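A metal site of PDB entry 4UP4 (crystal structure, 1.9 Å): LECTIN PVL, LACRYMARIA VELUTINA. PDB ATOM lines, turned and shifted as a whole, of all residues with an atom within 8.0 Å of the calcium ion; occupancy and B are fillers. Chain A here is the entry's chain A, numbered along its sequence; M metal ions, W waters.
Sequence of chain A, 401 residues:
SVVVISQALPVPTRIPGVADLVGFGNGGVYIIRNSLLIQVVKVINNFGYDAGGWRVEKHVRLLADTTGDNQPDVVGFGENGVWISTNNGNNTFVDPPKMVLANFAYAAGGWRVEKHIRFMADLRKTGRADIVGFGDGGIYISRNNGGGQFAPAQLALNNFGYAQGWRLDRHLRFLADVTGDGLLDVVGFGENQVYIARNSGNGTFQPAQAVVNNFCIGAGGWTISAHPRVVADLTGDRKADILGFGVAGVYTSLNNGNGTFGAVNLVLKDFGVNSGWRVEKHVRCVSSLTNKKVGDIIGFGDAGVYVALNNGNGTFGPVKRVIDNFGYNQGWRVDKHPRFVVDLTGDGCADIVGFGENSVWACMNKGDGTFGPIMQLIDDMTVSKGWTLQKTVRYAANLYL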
ATOM      1  N   ILE A  15      16.698  -6.117  32.961  1.00  0.00           N
ATOM      2  CA  ILE A  15      17.761  -6.057  31.943  1.00  0.00           C
ATOM      3  C   ILE A  15      19.055  -5.796  32.695  1.00  0.00           C
ATOM      4  O   ILE A  15      19.163  -4.773  33.341  1.00  0.00           O
ATOM      5  CB  ILE A  15      17.565  -4.860  31.006  1.00  0.00           C
ATOM      6  CG1 ILE A  15      16.327  -5.042  30.147  1.00  0.00           C
ATOM      7  CG2 ILE A  15      18.827  -4.611  30.148  1.00  0.00           C
ATOM      8  CD1 ILE A  15      16.421  -6.093  29.056  1.00  0.00           C
ATOM      9  N   PRO A  16      19.990  -6.731  32.719  1.00  0.00           N
ATOM     10  CA  PRO A  16      19.937  -8.058  32.201  1.00  0.00           C
ATOM     11  C   PRO A  16      19.079  -8.987  33.081  1.00  0.00           C
ATOM     12  O   PRO A  16      18.807  -8.697  34.250  1.00  0.00           O
ATOM     13  CB  PRO A  16      21.389  -8.512  32.242  1.00  0.00           C
ATOM     14  CG  PRO A  16      21.886  -7.876  33.483  1.00  0.00           C
ATOM     15  CD  PRO A  16      21.243  -6.519  33.483  1.00  0.00           C
ATOM     16  N   GLY A  17      18.699 -10.086  32.478  1.00  0.00           N
ATOM     17  CA  GLY A  17      17.968 -11.129  33.177  1.00  0.00           C
ATOM     18  C   GLY A  17      17.821 -12.395  32.340  1.00  0.00           C
ATOM     19  O   GLY A  17      18.080 -12.400  31.110  1.00  0.00           O
ATOM     20  N   VAL A  18      17.340 -13.424  33.026  1.00  0.00           N
ATOM     21  CA  VAL A  18      16.985 -14.674  32.380  1.00  0.00           C
ATOM     22  C   VAL A  18      15.557 -14.960  32.776  1.00  0.00           C
ATOM     23  O   VAL A  18      15.278 -15.759  33.664  1.00  0.00           O
ATOM     24  CB  VAL A  18      17.965 -15.817  32.778  1.00  0.00           C
ATOM     25  CG1 VAL A  18      19.323 -15.608  32.094  1.00  0.00           C
ATOM     26  CG2 VAL A  18      18.183 -15.846  34.284  1.00  0.00           C
ATOM     27  N   SER A 288      15.356  -2.588  25.290  1.00  0.00           N
ATOM     28  CA  SER A 288      16.789  -2.472  25.012  1.00  0.00           C
ATOM     29  C   SER A 288      17.331  -3.736  24.335  1.00  0.00           C
ATOM     30  O   SER A 288      17.309  -4.820  24.934  1.00  0.00           O
ATOM     31  CB  SER A 288      17.547  -2.214  26.279  1.00  0.00           C
ATOM     32  OG  SER A 288      18.939  -2.138  25.940  1.00  0.00           O
ATOM     33  N   LEU A 289      17.830  -3.577  23.116  1.00  0.00           N
ATOM     34  CA  LEU A 289      18.337  -4.678  22.311  1.00  0.00           C
ATOM     35  C   LEU A 289      19.869  -4.603  22.128  1.00  0.00           C
ATOM     36  O   LEU A 289      20.460  -5.502  21.542  1.00  0.00           O
ATOM     37  CB  LEU A 289      17.690  -4.691  20.930  1.00  0.00           C
ATOM     38  CG  LEU A 289      16.165  -4.792  20.891  1.00  0.00           C
ATOM     39  CD1 LEU A 289      15.683  -4.727  19.446  1.00  0.00           C
ATOM     40  CD2 LEU A 289      15.664  -6.022  21.603  1.00  0.00           C
ATOM     41  N   VAL A 342      12.049  -9.521  25.886  1.00  0.00           N
ATOM     42  CA  VAL A 342      12.546  -9.733  27.234  1.00  0.00           C
ATOM     43  C   VAL A 342      13.872 -10.483  27.172  1.00  0.00           C
ATOM     44  O   VAL A 342      14.064 -11.324  26.290  1.00  0.00           O
ATOM     45  CB  VAL A 342      11.491 -10.539  28.071  1.00  0.00           C
ATOM     46  CG1 VAL A 342      11.201 -11.867  27.432  1.00  0.00           C
ATOM     47  CG2 VAL A 342      11.944 -10.754  29.474  1.00  0.00           C
ATOM     48  N   ASP A 343      14.804 -10.115  28.064  1.00  0.00           N
ATOM     49  CA  ASP A 343      16.105 -10.829  28.163  1.00  0.00           C
ATOM     50  C   ASP A 343      15.870 -12.189  28.750  1.00  0.00           C
ATOM     51  O   ASP A 343      15.313 -12.306  29.856  1.00  0.00           O
ATOM     52  CB  ASP A 343      17.134 -10.082  28.984  1.00  0.00           C
ATOM     53  CG  ASP A 343      18.581 -10.525  28.715  1.00  0.00           C
ATOM     54  OD1 ASP A 343      18.851 -11.387  27.851  1.00  0.00           O
ATOM     55  OD2 ASP A 343      19.431 -10.035  29.492  1.00  0.00           O
ATOM     56  N   LEU A 344      16.208 -13.196  27.958  1.00  0.00           N
ATOM     57  CA  LEU A 344      16.148 -14.594  28.343  1.00  0.00           C
ATOM     58  C   LEU A 344      17.470 -15.266  28.578  1.00  0.00           C
ATOM     59  O   LEU A 344      17.496 -16.432  28.965  1.00  0.00           O
ATOM     60  CB  LEU A 344      15.400 -15.360  27.253  1.00  0.00           C
ATOM     61  CG  LEU A 344      13.939 -14.930  27.008  1.00  0.00           C
ATOM     62  CD1 LEU A 344      13.458 -15.570  25.703  1.00  0.00           C
ATOM     63  CD2 LEU A 344      13.012 -15.279  28.147  1.00  0.00           C
ATOM     64  N   THR A 345      18.544 -14.550  28.249  1.00  0.00           N
ATOM     65  CA  THR A 345      19.879 -15.094  28.188  1.00  0.00           C
ATOM     66  C   THR A 345      20.916 -14.467  29.180  1.00  0.00           C
ATOM     67  O   THR A 345      21.989 -15.026  29.343  1.00  0.00           O
ATOM     68  CB  THR A 345      20.478 -14.996  26.773  1.00  0.00           C
ATOM     69  OG1 THR A 345      20.807 -13.650  26.467  1.00  0.00           O
ATOM     70  CG2 THR A 345      19.464 -15.538  25.733  1.00  0.00           C
ATOM     71  N   GLY A 346      20.604 -13.320  29.792  1.00  0.00           N
ATOM     72  CA  GLY A 346      21.382 -12.690  30.819  1.00  0.00           C
ATOM     73  C   GLY A 346      22.459 -11.730  30.311  1.00  0.00           C
ATOM     74  O   GLY A 346      23.286 -11.279  31.076  1.00  0.00           O
ATOM     75  N   ASP A 347      22.475 -11.429  29.013  1.00  0.00           N
ATOM     76  CA  ASP A 347      23.521 -10.548  28.464  1.00  0.00           C
ATOM     77  C   ASP A 347      23.087  -9.049  28.427  1.00  0.00           C
ATOM     78  O   ASP A 347      23.824  -8.182  28.009  1.00  0.00           O
ATOM     79  CB  ASP A 347      23.929 -11.020  27.062  1.00  0.00           C
ATOM     80  CG  ASP A 347      22.836 -10.772  26.026  1.00  0.00           C
ATOM     81  OD1 ASP A 347      21.618 -10.737  26.411  1.00  0.00           O
ATOM     82  OD2 ASP A 347      23.181 -10.626  24.846  1.00  0.00           O
ATOM     83  N   GLY A 348      21.881  -8.767  28.878  1.00  0.00           N
ATOM     84  CA  GLY A 348      21.373  -7.385  28.843  1.00  0.00           C
ATOM     85  C   GLY A 348      20.752  -6.990  27.516  1.00  0.00           C
ATOM     86  O   GLY A 348      20.362  -5.846  27.332  1.00  0.00           O
ATOM     87  N   CYS A 349      20.658  -7.919  26.562  1.00  0.00           N
ATOM     88  CA  CYS A 349      20.085  -7.600  25.259  1.00  0.00           C
ATOM     89  C   CYS A 349      18.801  -8.368  25.105  1.00  0.00           C
ATOM     90  O   CYS A 349      18.778  -9.589  25.133  1.00  0.00           O
ATOM     91  CB  CYS A 349      21.070  -7.934  24.161  1.00  0.00           C
ATOM     92  SG  CYS A 349      22.540  -6.913  24.118  1.00  0.00           S
ATOM     93  N   ALA A 350      17.673  -7.653  24.964  1.00  0.00           N
ATOM     94  CA  ALA A 350      16.382  -8.338  25.003  1.00  0.00           C
ATOM     95  C   ALA A 350      16.232  -9.344  23.847  1.00  0.00           C
ATOM     96  O   ALA A 350      16.733  -9.121  22.733  1.00  0.00           O
ATOM     97  CB  ALA A 350      15.227  -7.351  25.039  1.00  0.00           C
ATOM     98  N   ASP A 351      15.557 -10.435  24.149  1.00  0.00           N
ATOM     99  CA  ASP A 351      15.274 -11.506  23.221  1.00  0.00           C
ATOM    100  C   ASP A 351      13.768 -11.521  22.896  1.00  0.00           C
ATOM    101  O   ASP A 351      13.043 -10.628  23.350  1.00  0.00           O
ATOM    102  CB  ASP A 351      15.750 -12.844  23.814  1.00  0.00           C
ATOM    103  CG  ASP A 351      17.156 -12.755  24.366  1.00  0.00           C
ATOM    104  OD1 ASP A 351      18.033 -12.499  23.518  1.00  0.00           O
ATOM    105  OD2 ASP A 351      17.415 -12.849  25.601  1.00  0.00           O
ATOM    106  N   ILE A 352      13.303 -12.513  22.138  1.00  0.00           N
ATOM    107  CA  ILE A 352      11.924 -12.651  21.727  1.00  0.00           C
ATOM    108  C   ILE A 352      11.388 -13.969  22.197  1.00  0.00           C
ATOM    109  O   ILE A 352      12.014 -14.998  22.046  1.00  0.00           O
ATOM    110  CB  ILE A 352      11.832 -12.554  20.234  1.00  0.00           C
ATOM    111  CG1 ILE A 352      12.328 -11.155  19.779  1.00  0.00           C
ATOM    112  CG2 ILE A 352      10.433 -12.849  19.767  1.00  0.00           C
ATOM    113  CD1 ILE A 352      12.659 -11.097  18.326  1.00  0.00           C
ATOM    114  N   CYS A 363      13.635 -16.577  20.142  1.00  0.00           N
ATOM    115  CA  CYS A 363      14.635 -16.211  19.216  1.00  0.00           C
ATOM    116  C   CYS A 363      15.573 -15.195  19.903  1.00  0.00           C
ATOM    117  O   CYS A 363      15.130 -14.179  20.454  1.00  0.00           O
ATOM    118  CB  CYS A 363      13.956 -15.660  17.991  1.00  0.00           C
ATOM    119  SG  CYS A 363      15.058 -14.977  16.795  1.00  0.00           S
ATOM    120  N   MET A 364      16.862 -15.528  19.909  1.00  0.00           N
ATOM    121  CA  MET A 364      17.826 -14.869  20.776  1.00  0.00           C
ATOM    122  C   MET A 364      18.631 -13.826  20.067  1.00  0.00           C
ATOM    123  O   MET A 364      19.113 -14.018  18.944  1.00  0.00           O
ATOM    124  CB  MET A 364      18.796 -15.868  21.442  1.00  0.00           C
ATOM    125  CG  MET A 364      18.085 -17.016  22.176  1.00  0.00           C
ATOM    126  SD  MET A 364      16.844 -16.417  23.294  1.00  0.00           S
ATOM    127  CE  MET A 364      16.255 -17.887  24.120  1.00  0.00           C
ATOM    128  N   ASN A 365      18.745 -12.703  20.758  1.00  0.00           N
ATOM    129  CA  ASN A 365      19.512 -11.557  20.318  1.00  0.00           C
ATOM    130  C   ASN A 365      20.974 -12.008  20.273  1.00  0.00           C
ATOM    131  O   ASN A 365      21.469 -12.649  21.187  1.00  0.00           O
ATOM    132  CB  ASN A 365      19.247 -10.393  21.291  1.00  0.00           C
ATOM    133  CG  ASN A 365      19.779  -9.042  20.847  1.00  0.00           C
ATOM    134  OD1 ASN A 365      20.875  -8.888  20.286  1.00  0.00           O
ATOM    135  ND2 ASN A 365      19.016  -8.010  21.206  1.00  0.00           N
ATOM    136  N   LYS A 366      21.675 -11.646  19.209  1.00  0.00           N
ATOM    137  CA  LYS A 366      23.093 -11.972  19.110  1.00  0.00           C
ATOM    138  C   LYS A 366      23.945 -11.134  19.994  1.00  0.00           C
ATOM    139  O   LYS A 366      25.141 -11.368  20.137  1.00  0.00           O
ATOM    140  CB  LYS A 366      23.532 -11.858  17.649  1.00  0.00           C
ATOM    141  CG  LYS A 366      22.925 -13.012  16.846  1.00  0.00           C
ATOM    142  CD  LYS A 366      23.188 -12.975  15.349  1.00  0.00           C
ATOM    143  CE  LYS A 366      22.769 -14.323  14.740  1.00  0.00           C
ATOM    144  NZ  LYS A 366      23.073 -14.413  13.288  1.00  0.00           N
ATOM    145  N   GLY A 367      23.383 -10.065  20.514  1.00  0.00           N
ATOM    146  CA  GLY A 367      24.106  -9.167  21.379  1.00  0.00           C
ATOM    147  C   GLY A 367      24.246  -7.784  20.770  1.00  0.00           C
ATOM    148  O   GLY A 367      24.784  -6.892  21.401  1.00  0.00           O
ATOM    149  N   PHE A 371      19.437 -11.061  15.344  1.00  0.00           N
ATOM    150  CA  PHE A 371      18.851 -12.227  16.005  1.00  0.00           C
ATOM    151  C   PHE A 371      19.226 -13.537  15.337  1.00  0.00           C
ATOM    152  O   PHE A 371      19.497 -13.593  14.139  1.00  0.00           O
ATOM    153  CB  PHE A 371      17.345 -12.099  16.091  1.00  0.00           C
ATOM    154  CG  PHE A 371      16.886 -11.068  17.112  1.00  0.00           C
ATOM    155  CD1 PHE A 371      17.058  -9.712  16.884  1.00  0.00           C
ATOM    156  CD2 PHE A 371      16.310 -11.477  18.306  1.00  0.00           C
ATOM    157  CE1 PHE A 371      16.654  -8.767  17.805  1.00  0.00           C
ATOM    158  CE2 PHE A 371      15.939 -10.523  19.267  1.00  0.00           C
ATOM    159  CZ  PHE A 371      16.089  -9.193  19.000  1.00  0.00           C
HETATM  160 CA    CA M   1      19.591 -11.712  25.583  1.00  0.00          CA
HETATM  161  O   HOH W   1      21.053 -11.744  23.766  1.00  0.00           O
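Five residues have an atom within 4 Å of the calcium ion: Asp 343, Thr 345, Asp 347, Cys 349 and Asp 351.
N of Asp 351 sits at hydrogen-bond distance from O of Val 342.
SG of Cys 349 is in hydrogen-bond range of O of Leu 289.
The side-chain sulfur of Cys 349 sits at hydrogen-bond distance from the backbone carbonyl oxygen of Gly 367 (3.5 Å).
The side-chain carboxylate of Asp 343 is in hydrogen-bond range of the backbone NH of Gly 17, 3.1 Å away.
The side-chain carboxylate (OD1) of Asp 343 lies close to the backbone NH (N) of Gly 346, 3.3 Å away.
The side-chain carboxylate of Asp 343 lies within hydrogen-bond range of the backbone NH of Gly 348 (2.8 Å).
OD1 of Asp 351 lies close to N of Asn 365, 2.9 Å away.
The side-chain carboxylate (OD2) of Asp 351 lies close to the backbone NH (N) of Leu 344 (2.7 Å).
The backbone carbonyl oxygen (O) of Cys 349 is bound to the calcium ion (2.3 Å).
The calcium ion is bound by water W1.
The calcium ion is bound by OD1 of Asp 347 (2.4 Å).
OD1 of Asp 343 binds the calcium ion (2.4 Å).
The side-chain hydroxyl (OG1) of Thr 345 binds the calcium ion (2.5 Å).
The calcium ion is bound by the side-chain carboxylate (OD2) of Asp 351.
OD1 of Asp 351 binds the calcium ion, at 2.7 Å.
Water W1 lies within hydrogen-bond range of the side-chain carboxylate (OD2) of Asp 347 (2.6 Å) and the backbone carbonyl oxygen (O) of Asn 365 (2.8 Å).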
